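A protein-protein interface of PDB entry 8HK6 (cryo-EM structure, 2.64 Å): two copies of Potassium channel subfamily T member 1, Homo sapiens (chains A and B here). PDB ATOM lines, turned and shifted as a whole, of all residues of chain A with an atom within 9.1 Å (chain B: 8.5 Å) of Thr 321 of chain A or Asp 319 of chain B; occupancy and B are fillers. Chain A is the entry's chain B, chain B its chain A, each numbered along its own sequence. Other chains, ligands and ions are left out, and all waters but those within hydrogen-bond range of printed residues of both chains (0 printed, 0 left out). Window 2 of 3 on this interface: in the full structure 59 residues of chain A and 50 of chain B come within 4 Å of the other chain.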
ATOM      1  N   PHE A 155      15.776  -2.177   2.761  1.00  0.00           N
ATOM      2  CA  PHE A 155      17.191  -1.870   2.624  1.00  0.00           C
ATOM      3  C   PHE A 155      17.363  -0.650   1.730  1.00  0.00           C
ATOM      4  O   PHE A 155      16.813  -0.603   0.624  1.00  0.00           O
ATOM      5  CB  PHE A 155      17.958  -3.062   2.048  1.00  0.00           C
ATOM      6  CG  PHE A 155      19.375  -2.746   1.670  1.00  0.00           C
ATOM      7  CD1 PHE A 155      20.298  -2.385   2.636  1.00  0.00           C
ATOM      8  CD2 PHE A 155      19.786  -2.815   0.350  1.00  0.00           C
ATOM      9  CE1 PHE A 155      21.604  -2.095   2.293  1.00  0.00           C
ATOM     10  CE2 PHE A 155      21.091  -2.526   0.001  1.00  0.00           C
ATOM     11  CZ  PHE A 155      22.001  -2.167   0.975  1.00  0.00           C
ATOM     12  N   ILE A 289      26.680 -15.838   4.924  1.00  0.00           N
ATOM     13  CA  ILE A 289      26.313 -14.853   3.911  1.00  0.00           C
ATOM     14  C   ILE A 289      24.807 -14.652   3.861  1.00  0.00           C
ATOM     15  O   ILE A 289      24.331 -13.513   3.809  1.00  0.00           O
ATOM     16  CB  ILE A 289      26.874 -15.257   2.536  1.00  0.00           C
ATOM     17  CG1 ILE A 289      28.398 -15.137   2.530  1.00  0.00           C
ATOM     18  CG2 ILE A 289      26.264 -14.408   1.433  1.00  0.00           C
ATOM     19  CD1 ILE A 289      28.885 -13.709   2.615  1.00  0.00           C
ATOM     20  N   GLU A 293      23.276 -11.073   5.068  1.00  0.00           N
ATOM     21  CA  GLU A 293      22.574 -10.369   4.005  1.00  0.00           C
ATOM     22  C   GLU A 293      21.070 -10.321   4.224  1.00  0.00           C
ATOM     23  O   GLU A 293      20.363  -9.717   3.412  1.00  0.00           O
ATOM     24  CB  GLU A 293      22.876 -11.013   2.651  1.00  0.00           C
ATOM     25  CG  GLU A 293      24.211 -10.602   2.055  1.00  0.00           C
ATOM     26  CD  GLU A 293      24.189  -9.196   1.491  1.00  0.00           C
ATOM     27  OE1 GLU A 293      23.786  -9.030   0.321  1.00  0.00           O
ATOM     28  OE2 GLU A 293      24.573  -8.256   2.217  1.00  0.00           O
ATOM     29  N   GLY A 296      20.471  -6.813   4.291  1.00  0.00           N
ATOM     30  CA  GLY A 296      20.602  -6.150   3.009  1.00  0.00           C
ATOM     31  C   GLY A 296      20.545  -7.081   1.813  1.00  0.00           C
ATOM     32  O   GLY A 296      21.379  -7.982   1.678  1.00  0.00           O
ATOM     33  N   GLU A 297      19.556  -6.855   0.943  1.00  0.00           N
ATOM     34  CA  GLU A 297      19.327  -7.573  -0.311  1.00  0.00           C
ATOM     35  C   GLU A 297      18.733  -8.965  -0.109  1.00  0.00           C
ATOM     36  O   GLU A 297      18.368  -9.622  -1.089  1.00  0.00           O
ATOM     37  CB  GLU A 297      20.617  -7.675  -1.133  1.00  0.00           C
ATOM     38  N   ASN A 298      18.614  -9.410   1.143  1.00  0.00           N
ATOM     39  CA  ASN A 298      17.849 -10.606   1.514  1.00  0.00           C
ATOM     40  C   ASN A 298      18.168 -11.802   0.610  1.00  0.00           C
ATOM     41  O   ASN A 298      17.315 -12.302  -0.126  1.00  0.00           O
ATOM     42  CB  ASN A 298      16.347 -10.308   1.501  1.00  0.00           C
ATOM     43  CG  ASN A 298      15.886  -9.580   2.743  1.00  0.00           C
ATOM     44  OD1 ASN A 298      14.755  -9.099   2.812  1.00  0.00           O
ATOM     45  ND2 ASN A 298      16.762  -9.487   3.732  1.00  0.00           N
ATOM     46  N   LEU A 299      19.418 -12.255   0.670  1.00  0.00           N
ATOM     47  CA  LEU A 299      19.832 -13.397  -0.136  1.00  0.00           C
ATOM     48  C   LEU A 299      19.162 -14.675   0.355  1.00  0.00           C
ATOM     49  O   LEU A 299      18.954 -14.858   1.557  1.00  0.00           O
ATOM     50  CB  LEU A 299      21.349 -13.557  -0.098  1.00  0.00           C
ATOM     51  CG  LEU A 299      22.166 -12.576  -0.935  1.00  0.00           C
ATOM     52  CD1 LEU A 299      23.647 -12.871  -0.790  1.00  0.00           C
ATOM     53  CD2 LEU A 299      21.743 -12.644  -2.391  1.00  0.00           C
ATOM     54  N   THR A 303      20.807 -18.988  -3.393  1.00  0.00           N
ATOM     55  CA  THR A 303      21.643 -17.957  -4.000  1.00  0.00           C
ATOM     56  C   THR A 303      22.962 -17.799  -3.256  1.00  0.00           C
ATOM     57  O   THR A 303      24.021 -17.700  -3.884  1.00  0.00           O
ATOM     58  CB  THR A 303      20.899 -16.624  -4.040  1.00  0.00           C
ATOM     59  OG1 THR A 303      19.676 -16.777  -4.770  1.00  0.00           O
ATOM     60  CG2 THR A 303      21.752 -15.564  -4.716  1.00  0.00           C
ATOM     61  N   SER A 304      22.921 -17.780  -1.922  1.00  0.00           N
ATOM     62  CA  SER A 304      24.153 -17.651  -1.152  1.00  0.00           C
ATOM     63  C   SER A 304      25.039 -18.878  -1.308  1.00  0.00           C
ATOM     64  O   SER A 304      26.268 -18.757  -1.278  1.00  0.00           O
ATOM     65  CB  SER A 304      23.837 -17.408   0.321  1.00  0.00           C
ATOM     66  OG  SER A 304      22.825 -18.284   0.775  1.00  0.00           O
ATOM     67  N   TYR A 306      25.365 -20.642  -4.056  1.00  0.00           N
ATOM     68  CA  TYR A 306      26.051 -20.415  -5.323  1.00  0.00           C
ATOM     69  C   TYR A 306      27.125 -19.345  -5.180  1.00  0.00           C
ATOM     70  O   TYR A 306      28.159 -19.398  -5.856  1.00  0.00           O
ATOM     71  CB  TYR A 306      25.029 -20.035  -6.394  1.00  0.00           C
ATOM     72  CG  TYR A 306      25.561 -19.215  -7.547  1.00  0.00           C
ATOM     73  CD1 TYR A 306      26.197 -19.820  -8.622  1.00  0.00           C
ATOM     74  CD2 TYR A 306      25.396 -17.837  -7.577  1.00  0.00           C
ATOM     75  CE1 TYR A 306      26.672 -19.074  -9.681  1.00  0.00           C
ATOM     76  CE2 TYR A 306      25.867 -17.085  -8.631  1.00  0.00           C
ATOM     77  CZ  TYR A 306      26.503 -17.707  -9.682  1.00  0.00           C
ATOM     78  OH  TYR A 306      26.974 -16.958 -10.734  1.00  0.00           O
ATOM     79  N   PHE A 307      26.897 -18.367  -4.303  1.00  0.00           N
ATOM     80  CA  PHE A 307      27.868 -17.295  -4.108  1.00  0.00           C
ATOM     81  C   PHE A 307      29.164 -17.820  -3.503  1.00  0.00           C
ATOM     82  O   PHE A 307      30.260 -17.423  -3.913  1.00  0.00           O
ATOM     83  CB  PHE A 307      27.265 -16.207  -3.223  1.00  0.00           C
ATOM     84  CG  PHE A 307      28.279 -15.270  -2.642  1.00  0.00           C
ATOM     85  CD1 PHE A 307      28.860 -14.290  -3.424  1.00  0.00           C
ATOM     86  CD2 PHE A 307      28.660 -15.375  -1.317  1.00  0.00           C
ATOM     87  CE1 PHE A 307      29.791 -13.428  -2.893  1.00  0.00           C
ATOM     88  CE2 PHE A 307      29.594 -14.518  -0.783  1.00  0.00           C
ATOM     89  CZ  PHE A 307      30.160 -13.543  -1.573  1.00  0.00           C
ATOM     90  N   VAL A 310      31.365 -20.072  -5.999  1.00  0.00           N
ATOM     91  CA  VAL A 310      32.149 -19.272  -6.939  1.00  0.00           C
ATOM     92  C   VAL A 310      33.135 -18.350  -6.242  1.00  0.00           C
ATOM     93  O   VAL A 310      33.992 -17.761  -6.909  1.00  0.00           O
ATOM     94  CB  VAL A 310      31.245 -18.437  -7.865  1.00  0.00           C
ATOM     95  CG1 VAL A 310      30.199 -19.321  -8.520  1.00  0.00           C
ATOM     96  CG2 VAL A 310      30.596 -17.303  -7.104  1.00  0.00           C
ATOM     97  N   THR A 311      33.039 -18.205  -4.920  1.00  0.00           N
ATOM     98  CA  THR A 311      34.044 -17.448  -4.181  1.00  0.00           C
ATOM     99  C   THR A 311      35.235 -18.323  -3.816  1.00  0.00           C
ATOM    100  O   THR A 311      36.383 -17.977  -4.114  1.00  0.00           O
ATOM    101  CB  THR A 311      33.432 -16.839  -2.919  1.00  0.00           C
ATOM    102  OG1 THR A 311      32.624 -15.710  -3.272  1.00  0.00           O
ATOM    103  CG2 THR A 311      34.523 -16.402  -1.953  1.00  0.00           C
ATOM    104  N   GLY A 316      34.563 -15.729  -8.720  1.00  0.00           N
ATOM    105  CA  GLY A 316      34.095 -14.385  -8.445  1.00  0.00           C
ATOM    106  C   GLY A 316      33.323 -13.748  -9.580  1.00  0.00           C
ATOM    107  O   GLY A 316      33.794 -12.784 -10.189  1.00  0.00           O
ATOM    108  N   TYR A 317      32.138 -14.284  -9.883  1.00  0.00           N
ATOM    109  CA  TYR A 317      31.325 -13.711 -10.952  1.00  0.00           C
ATOM    110  C   TYR A 317      30.929 -12.276 -10.635  1.00  0.00           C
ATOM    111  O   TYR A 317      31.019 -11.394 -11.496  1.00  0.00           O
ATOM    112  CB  TYR A 317      30.079 -14.563 -11.185  1.00  0.00           C
ATOM    113  CG  TYR A 317      30.328 -15.819 -11.980  1.00  0.00           C
ATOM    114  CD1 TYR A 317      30.179 -17.069 -11.402  1.00  0.00           C
ATOM    115  CD2 TYR A 317      30.714 -15.753 -13.309  1.00  0.00           C
ATOM    116  CE1 TYR A 317      30.404 -18.218 -12.127  1.00  0.00           C
ATOM    117  CE2 TYR A 317      30.943 -16.895 -14.039  1.00  0.00           C
ATOM    118  CZ  TYR A 317      30.788 -18.124 -13.444  1.00  0.00           C
ATOM    119  OH  TYR A 317      31.013 -19.266 -14.173  1.00  0.00           O
ATOM    120  N   GLY A 318      30.498 -12.021  -9.405  1.00  0.00           N
ATOM    121  CA  GLY A 318      30.071 -10.700  -9.010  1.00  0.00           C
ATOM    122  C   GLY A 318      28.614 -10.388  -9.264  1.00  0.00           C
ATOM    123  O   GLY A 318      28.180  -9.268  -8.964  1.00  0.00           O
ATOM    124  N   ASP A 319      27.841 -11.329  -9.811  1.00  0.00           N
ATOM    125  CA  ASP A 319      26.412 -11.084  -9.971  1.00  0.00           C
ATOM    126  C   ASP A 319      25.709 -11.017  -8.621  1.00  0.00           C
ATOM    127  O   ASP A 319      24.730 -10.279  -8.470  1.00  0.00           O
ATOM    128  CB  ASP A 319      25.789 -12.145 -10.886  1.00  0.00           C
ATOM    129  CG  ASP A 319      25.883 -13.555 -10.325  1.00  0.00           C
ATOM    130  OD1 ASP A 319      26.327 -14.454 -11.068  1.00  0.00           O
ATOM    131  OD2 ASP A 319      25.478 -13.785  -9.169  1.00  0.00           O
ATOM    132  N   VAL A 320      26.190 -11.773  -7.637  1.00  0.00           N
ATOM    133  CA  VAL A 320      25.782 -11.618  -6.246  1.00  0.00           C
ATOM    134  C   VAL A 320      27.033 -11.255  -5.457  1.00  0.00           C
ATOM    135  O   VAL A 320      28.003 -12.021  -5.433  1.00  0.00           O
ATOM    136  CB  VAL A 320      25.117 -12.880  -5.677  1.00  0.00           C
ATOM    137  CG1 VAL A 320      25.859 -14.133  -6.106  1.00  0.00           C
ATOM    138  CG2 VAL A 320      25.048 -12.799  -4.164  1.00  0.00           C
ATOM    139  N   THR A 321      27.023 -10.084  -4.832  1.00  0.00           N
ATOM    140  CA  THR A 321      28.152  -9.603  -4.056  1.00  0.00           C
ATOM    141  C   THR A 321      27.654  -9.003  -2.751  1.00  0.00           C
ATOM    142  O   THR A 321      26.546  -8.459  -2.696  1.00  0.00           O
ATOM    143  CB  THR A 321      28.956  -8.556  -4.842  1.00  0.00           C
ATOM    144  OG1 THR A 321      29.904  -7.918  -3.979  1.00  0.00           O
ATOM    145  CG2 THR A 321      28.033  -7.510  -5.437  1.00  0.00           C
ATOM    146  N   PRO A 322      28.439  -9.103  -1.678  1.00  0.00           N
ATOM    147  CA  PRO A 322      28.024  -8.497  -0.407  1.00  0.00           C
ATOM    148  C   PRO A 322      27.908  -6.984  -0.529  1.00  0.00           C
ATOM    149  O   PRO A 322      28.856  -6.300  -0.922  1.00  0.00           O
ATOM    150  CB  PRO A 322      29.140  -8.908   0.561  1.00  0.00           C
ATOM    151  CG  PRO A 322      30.299  -9.261  -0.313  1.00  0.00           C
ATOM    152  CD  PRO A 322      29.697  -9.855  -1.541  1.00  0.00           C
ATOM    153  N   LYS A 323      26.731  -6.464  -0.186  1.00  0.00           N
ATOM    154  CA  LYS A 323      26.424  -5.049  -0.335  1.00  0.00           C
ATOM    155  C   LYS A 323      26.543  -4.261   0.962  1.00  0.00           C
ATOM    156  O   LYS A 323      26.332  -3.045   0.949  1.00  0.00           O
ATOM    157  CB  LYS A 323      25.014  -4.874  -0.906  1.00  0.00           C
ATOM    158  CG  LYS A 323      24.686  -5.803  -2.060  1.00  0.00           C
ATOM    159  CD  LYS A 323      24.106  -5.030  -3.232  1.00  0.00           C
ATOM    160  CE  LYS A 323      23.736  -5.958  -4.378  1.00  0.00           C
ATOM    161  NZ  LYS A 323      24.930  -6.391  -5.151  1.00  0.00           N
ATOM    162  N   ILE A 324      26.872  -4.912   2.076  1.00  0.00           N
ATOM    163  CA  ILE A 324      27.003  -4.238   3.359  1.00  0.00           C
ATOM    164  C   ILE A 324      28.322  -4.650   3.997  1.00  0.00           C
ATOM    165  O   ILE A 324      28.847  -5.736   3.746  1.00  0.00           O
ATOM    166  CB  ILE A 324      25.827  -4.550   4.306  1.00  0.00           C
ATOM    167  CG1 ILE A 324      25.675  -6.058   4.493  1.00  0.00           C
ATOM    168  CG2 ILE A 324      24.541  -3.940   3.776  1.00  0.00           C
ATOM    169  CD1 ILE A 324      24.529  -6.438   5.397  1.00  0.00           C
ATOM    170  N   SER A 327      28.735  -8.076   5.718  1.00  0.00           N
ATOM    171  CA  SER A 327      28.851  -9.182   4.774  1.00  0.00           C
ATOM    172  C   SER A 327      30.193  -9.149   4.053  1.00  0.00           C
ATOM    173  O   SER A 327      30.801 -10.196   3.806  1.00  0.00           O
ATOM    174  CB  SER A 327      27.697  -9.140   3.775  1.00  0.00           C
ATOM    175  OG  SER A 327      26.489  -9.563   4.378  1.00  0.00           O
ATOM    176  N   GLN A 328      30.666  -7.952   3.701  1.00  0.00           N
ATOM    177  CA  GLN A 328      31.970  -7.826   3.057  1.00  0.00           C
ATOM    178  C   GLN A 328      33.083  -8.309   3.976  1.00  0.00           C
ATOM    179  O   GLN A 328      34.011  -9.000   3.540  1.00  0.00           O
ATOM    180  CB  GLN A 328      32.213  -6.376   2.639  1.00  0.00           C
ATOM    181  CG  GLN A 328      31.214  -5.837   1.633  1.00  0.00           C
ATOM    182  CD  GLN A 328      31.496  -4.399   1.250  1.00  0.00           C
ATOM    183  OE1 GLN A 328      32.058  -3.636   2.034  1.00  0.00           O
ATOM    184  NE2 GLN A 328      31.107  -4.022   0.039  1.00  0.00           N
ATOM    185  N   VAL A 331      33.163 -12.130   4.163  1.00  0.00           N
ATOM    186  CA  VAL A 331      33.832 -12.721   3.009  1.00  0.00           C
ATOM    187  C   VAL A 331      35.343 -12.634   3.164  1.00  0.00           C
ATOM    188  O   VAL A 331      36.062 -13.592   2.860  1.00  0.00           O
ATOM    189  CB  VAL A 331      33.350 -12.041   1.715  1.00  0.00           C
ATOM    190  CG1 VAL A 331      34.429 -12.083   0.645  1.00  0.00           C
ATOM    191  CG2 VAL A 331      32.085 -12.702   1.218  1.00  0.00           C
ATOM    192  N   LEU B 299      36.778   6.047  -2.387  1.00  0.00           N
ATOM    193  CA  LEU B 299      36.646   4.794  -1.655  1.00  0.00           C
ATOM    194  C   LEU B 299      37.028   4.978  -0.190  1.00  0.00           C
ATOM    195  O   LEU B 299      37.940   5.742   0.134  1.00  0.00           O
ATOM    196  CB  LEU B 299      37.525   3.720  -2.291  1.00  0.00           C
ATOM    197  CG  LEU B 299      36.890   2.354  -2.547  1.00  0.00           C
ATOM    198  CD1 LEU B 299      35.458   2.502  -3.031  1.00  0.00           C
ATOM    199  CD2 LEU B 299      37.722   1.577  -3.549  1.00  0.00           C
ATOM    200  N   THR B 303      36.112  -0.256   2.579  1.00  0.00           N
ATOM    201  CA  THR B 303      35.786  -0.763   1.252  1.00  0.00           C
ATOM    202  C   THR B 303      37.042  -1.118   0.468  1.00  0.00           C
ATOM    203  O   THR B 303      37.087  -2.162  -0.191  1.00  0.00           O
ATOM    204  CB  THR B 303      34.952   0.261   0.487  1.00  0.00           C
ATOM    205  OG1 THR B 303      33.782   0.589   1.246  1.00  0.00           O
ATOM    206  CG2 THR B 303      34.527  -0.306  -0.853  1.00  0.00           C
ATOM    207  N   TYR B 306      38.498  -4.419   1.592  1.00  0.00           N
ATOM    208  CA  TYR B 306      37.778  -5.542   1.001  1.00  0.00           C
ATOM    209  C   TYR B 306      38.158  -5.726  -0.462  1.00  0.00           C
ATOM    210  O   TYR B 306      38.196  -6.855  -0.964  1.00  0.00           O
ATOM    211  CB  TYR B 306      36.273  -5.321   1.160  1.00  0.00           C
ATOM    212  CG  TYR B 306      35.404  -6.021   0.142  1.00  0.00           C
ATOM    213  CD1 TYR B 306      35.066  -7.358   0.289  1.00  0.00           C
ATOM    214  CD2 TYR B 306      34.895  -5.335  -0.951  1.00  0.00           C
ATOM    215  CE1 TYR B 306      34.263  -7.996  -0.631  1.00  0.00           C
ATOM    216  CE2 TYR B 306      34.092  -5.964  -1.877  1.00  0.00           C
ATOM    217  CZ  TYR B 306      33.778  -7.294  -1.714  1.00  0.00           C
ATOM    218  OH  TYR B 306      32.976  -7.923  -2.637  1.00  0.00           O
ATOM    219  N   PHE B 307      38.443  -4.627  -1.162  1.00  0.00           N
ATOM    220  CA  PHE B 307      38.824  -4.710  -2.567  1.00  0.00           C
ATOM    221  C   PHE B 307      40.147  -5.449  -2.742  1.00  0.00           C
ATOM    222  O   PHE B 307      40.300  -6.261  -3.660  1.00  0.00           O
ATOM    223  CB  PHE B 307      38.908  -3.306  -3.163  1.00  0.00           C
ATOM    224  CG  PHE B 307      39.660  -3.241  -4.458  1.00  0.00           C
ATOM    225  CD1 PHE B 307      39.081  -3.680  -5.633  1.00  0.00           C
ATOM    226  CD2 PHE B 307      40.950  -2.742  -4.500  1.00  0.00           C
ATOM    227  CE1 PHE B 307      39.771  -3.619  -6.824  1.00  0.00           C
ATOM    228  CE2 PHE B 307      41.642  -2.680  -5.688  1.00  0.00           C
ATOM    229  CZ  PHE B 307      41.054  -3.119  -6.850  1.00  0.00           C
ATOM    230  N   VAL B 310      39.971  -9.389  -1.959  1.00  0.00           N
ATOM    231  CA  VAL B 310      39.407 -10.145  -3.076  1.00  0.00           C
ATOM    232  C   VAL B 310      40.220  -9.998  -4.352  1.00  0.00           C
ATOM    233  O   VAL B 310      39.977 -10.734  -5.315  1.00  0.00           O
ATOM    234  CB  VAL B 310      37.949  -9.733  -3.355  1.00  0.00           C
ATOM    235  CG1 VAL B 310      37.146  -9.739  -2.068  1.00  0.00           C
ATOM    236  CG2 VAL B 310      37.893  -8.375  -4.024  1.00  0.00           C
ATOM    237  N   GLY B 316      38.184 -11.279  -7.397  1.00  0.00           N
ATOM    238  CA  GLY B 316      37.790 -10.190  -8.268  1.00  0.00           C
ATOM    239  C   GLY B 316      36.305 -10.111  -8.553  1.00  0.00           C
ATOM    240  O   GLY B 316      35.876 -10.370  -9.681  1.00  0.00           O
ATOM    241  N   TYR B 317      35.506  -9.771  -7.538  1.00  0.00           N
ATOM    242  CA  TYR B 317      34.067  -9.655  -7.747  1.00  0.00           C
ATOM    243  C   TYR B 317      33.742  -8.582  -8.776  1.00  0.00           C
ATOM    244  O   TYR B 317      32.885  -8.783  -9.643  1.00  0.00           O
ATOM    245  CB  TYR B 317      33.355  -9.350  -6.431  1.00  0.00           C
ATOM    246  CG  TYR B 317      33.408 -10.463  -5.416  1.00  0.00           C
ATOM    247  CD1 TYR B 317      32.556 -11.550  -5.511  1.00  0.00           C
ATOM    248  CD2 TYR B 317      34.286 -10.412  -4.344  1.00  0.00           C
ATOM    249  CE1 TYR B 317      32.593 -12.565  -4.588  1.00  0.00           C
ATOM    250  CE2 TYR B 317      34.326 -11.423  -3.411  1.00  0.00           C
ATOM    251  CZ  TYR B 317      33.477 -12.497  -3.539  1.00  0.00           C
ATOM    252  OH  TYR B 317      33.511 -13.508  -2.613  1.00  0.00           O
ATOM    253  N   GLY B 318      34.416  -7.440  -8.700  1.00  0.00           N
ATOM    254  CA  GLY B 318      34.146  -6.347  -9.604  1.00  0.00           C
ATOM    255  C   GLY B 318      33.090  -5.373  -9.137  1.00  0.00           C
ATOM    256  O   GLY B 318      32.815  -4.399  -9.850  1.00  0.00           O
ATOM    257  N   ASP B 319      32.480  -5.602  -7.972  1.00  0.00           N
ATOM    258  CA  ASP B 319      31.566  -4.610  -7.417  1.00  0.00           C
ATOM    259  C   ASP B 319      32.288  -3.309  -7.105  1.00  0.00           C
ATOM    260  O   ASP B 319      31.706  -2.227  -7.244  1.00  0.00           O
ATOM    261  CB  ASP B 319      30.884  -5.160  -6.164  1.00  0.00           C
ATOM    262  CG  ASP B 319      31.872  -5.562  -5.087  1.00  0.00           C
ATOM    263  OD1 ASP B 319      33.092  -5.545  -5.352  1.00  0.00           O
ATOM    264  OD2 ASP B 319      31.428  -5.893  -3.968  1.00  0.00           O
ATOM    265  N   VAL B 320      33.546  -3.395  -6.683  1.00  0.00           N
ATOM    266  CA  VAL B 320      34.405  -2.236  -6.486  1.00  0.00           C
ATOM    267  C   VAL B 320      35.611  -2.432  -7.395  1.00  0.00           C
ATOM    268  O   VAL B 320      36.354  -3.410  -7.247  1.00  0.00           O
ATOM    269  CB  VAL B 320      34.835  -2.073  -5.021  1.00  0.00           C
ATOM    270  CG1 VAL B 320      36.179  -1.370  -4.925  1.00  0.00           C
ATOM    271  CG2 VAL B 320      33.773  -1.314  -4.247  1.00  0.00           C
ATOM    272  N   THR B 321      35.790  -1.526  -8.349  1.00  0.00           N
ATOM    273  CA  THR B 321      36.889  -1.595  -9.295  1.00  0.00           C
ATOM    274  C   THR B 321      37.474  -0.208  -9.510  1.00  0.00           C
ATOM    275  O   THR B 321      36.756   0.792  -9.422  1.00  0.00           O
ATOM    276  CB  THR B 321      36.426  -2.187 -10.637  1.00  0.00           C
ATOM    277  OG1 THR B 321      37.443  -2.007 -11.631  1.00  0.00           O
ATOM    278  CG2 THR B 321      35.137  -1.538 -11.100  1.00  0.00           C
ATOM    279  N   PRO B 322      38.777  -0.119  -9.770  1.00  0.00           N
ATOM    280  CA  PRO B 322      39.386   1.192 -10.029  1.00  0.00           C
ATOM    281  C   PRO B 322      38.792   1.842 -11.270  1.00  0.00           C
ATOM    282  O   PRO B 322      38.730   1.235 -12.341  1.00  0.00           O
ATOM    283  CB  PRO B 322      40.871   0.859 -10.215  1.00  0.00           C
ATOM    284  CG  PRO B 322      40.902  -0.600 -10.542  1.00  0.00           C
ATOM    285  CD  PRO B 322      39.780  -1.195  -9.762  1.00  0.00           C
ATOM    286  N   LYS B 323      38.358   3.091 -11.116  1.00  0.00           N
ATOM    287  CA  LYS B 323      37.680   3.823 -12.177  1.00  0.00           C
ATOM    288  C   LYS B 323      38.571   4.841 -12.876  1.00  0.00           C
ATOM    289  O   LYS B 323      38.128   5.465 -13.843  1.00  0.00           O
ATOM    290  CB  LYS B 323      36.446   4.540 -11.619  1.00  0.00           C
ATOM    291  CG  LYS B 323      35.595   3.714 -10.671  1.00  0.00           C
ATOM    292  CD  LYS B 323      34.228   3.428 -11.272  1.00  0.00           C
ATOM    293  CE  LYS B 323      33.354   2.628 -10.320  1.00  0.00           C
ATOM    294  NZ  LYS B 323      33.555   1.165 -10.452  1.00  0.00           N
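Thr 321 of chain A touches two residues of chain B. Printed residues of chain A within 4 Å of Asp 319 of chain B: Thr 321. No residue of chain B comes within 4 Å of Val 320 of chain A. No residue of chain A comes within 4 Å of Val 320 of chain B. Of the printed residues of chain B, Pro 322 of chain A touches Tyr 306 (3.8 Å). Of the printed residues of chain B, Gly 318 of chain A touches Tyr 317 (3.5 Å). Printed residues of chain B within 4 Å of Thr 311 of chain A: Tyr 317 (2.5 Å). Of the printed residues of chain A, Gly 316 of chain B touches Gly 316 (3.2 Å). Leu 299 of chain B touches none of the printed residues of chain A. The nearest residue of chain B that does not touch Thr 321 of chain A is Tyr 317 of chain B (4.5 Å). The nearest printed residue of chain A that does not touch Asp 319 of chain B is Pro 322 of chain A (4.01 Å). The nearest printed residue of chain A that does not touch Tyr 317 of chain B is Thr 321 of chain A (4.5 Å).
CE1 of Phe 307 of chain A touches CE1 of Tyr 317 of chain B, at 3.4 Å. Tyr 317 of chain B touches Gly 316 of chain A (CA to O, 3.98 Å). Tyr 317 of chain B touches Tyr 317 of chain A. Gly 318 of chain A touches Tyr 317 of chain B (CA to O, 3.5 Å). Pro 322 of chain A touches Tyr 306 of chain B (CG to OH, 3.8 Å). Gln 328 of chain A touches Tyr 306 of chain B. CG1 of Val 331 of chain A touches OH of Tyr 317 of chain B, 3.7 Å away.
The backbone carbonyl oxygen of Phe 307 of chain A sits at hydrogen-bond distance from the side-chain hydroxyl of Thr 311 of chain A, 3.0 Å away. O of Val 310 of chain B is in hydrogen-bond range of N of Gly 316 of chain B, at 2.8 Å. The backbone NH of Gly 316 of chain A is in hydrogen-bond range of the backbone carbonyl oxygen of Val 310 of chain A, 2.8 Å away. O of Pro 322 of chain A lies within hydrogen-bond range of NE2 of Gln 328 of chain A (3.3 Å). The side-chain hydroxyl (OH) of Tyr 306 of chain B is in hydrogen-bond range of the side-chain carboxylate (OD2) of Asp 319 of chain B, at 2.9 Å.
Of the 25 printed residues of chain A, 9 touch a printed residue of chain B. Hydrophobic or aromatic side chains of chain A within 4 Å of the printed part of chain B: Phe 307, Pro 322 and Val 331. Along chain B the printed residues that touch a printed residue of chain A span positions 306 to 319. Among the printed residues, 11 pairs touch across the chains. Among the printed residues, no Asp or Glu carboxylate lies within 4 Å of a Lys or Arg side-chain nitrogen of the other chain.
Gly 316 of chain A touches Tyr 317 of chain B, but with the chains exchanged Tyr 317 of chain A does not touch Gly 316 of chain B (5.3 Å). Tyr 317 of chain A touches its own counterpart, Tyr 317 of chain B. Thr 321 of chain A touches Tyr 306 of chain B, but with the chains exchanged Tyr 306 of chain A does not touch Thr 321 of chain B (17.5 Å). Thr 321 of chain A touches Asp 319 of chain B, but with the chains exchanged Asp 319 of chain A does not touch Thr 321 of chain B (12.3 Å). 13 positions are printed for both chains.
The backbone carbonyl oxygen (O) of Gly 316 of chain B lies close to the backbone carbonyl oxygen (O) of Gly 316 of chain A, at 3.2 Å. The side-chain hydroxyl (OH) of Tyr 317 of chain B sits at hydrogen-bond distance from the side-chain hydroxyl (OG1) of Thr 311 of chain A, 2.5 Å away. The side-chain hydroxyl of Thr 321 of chain A lies within hydrogen-bond range of the side-chain carboxylate of Asp 319 of chain B (2.5 Å). OG1 of Thr 321 of chain A is in hydrogen-bond range of OH of Tyr 306 of chain B, at 3.4 Å.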
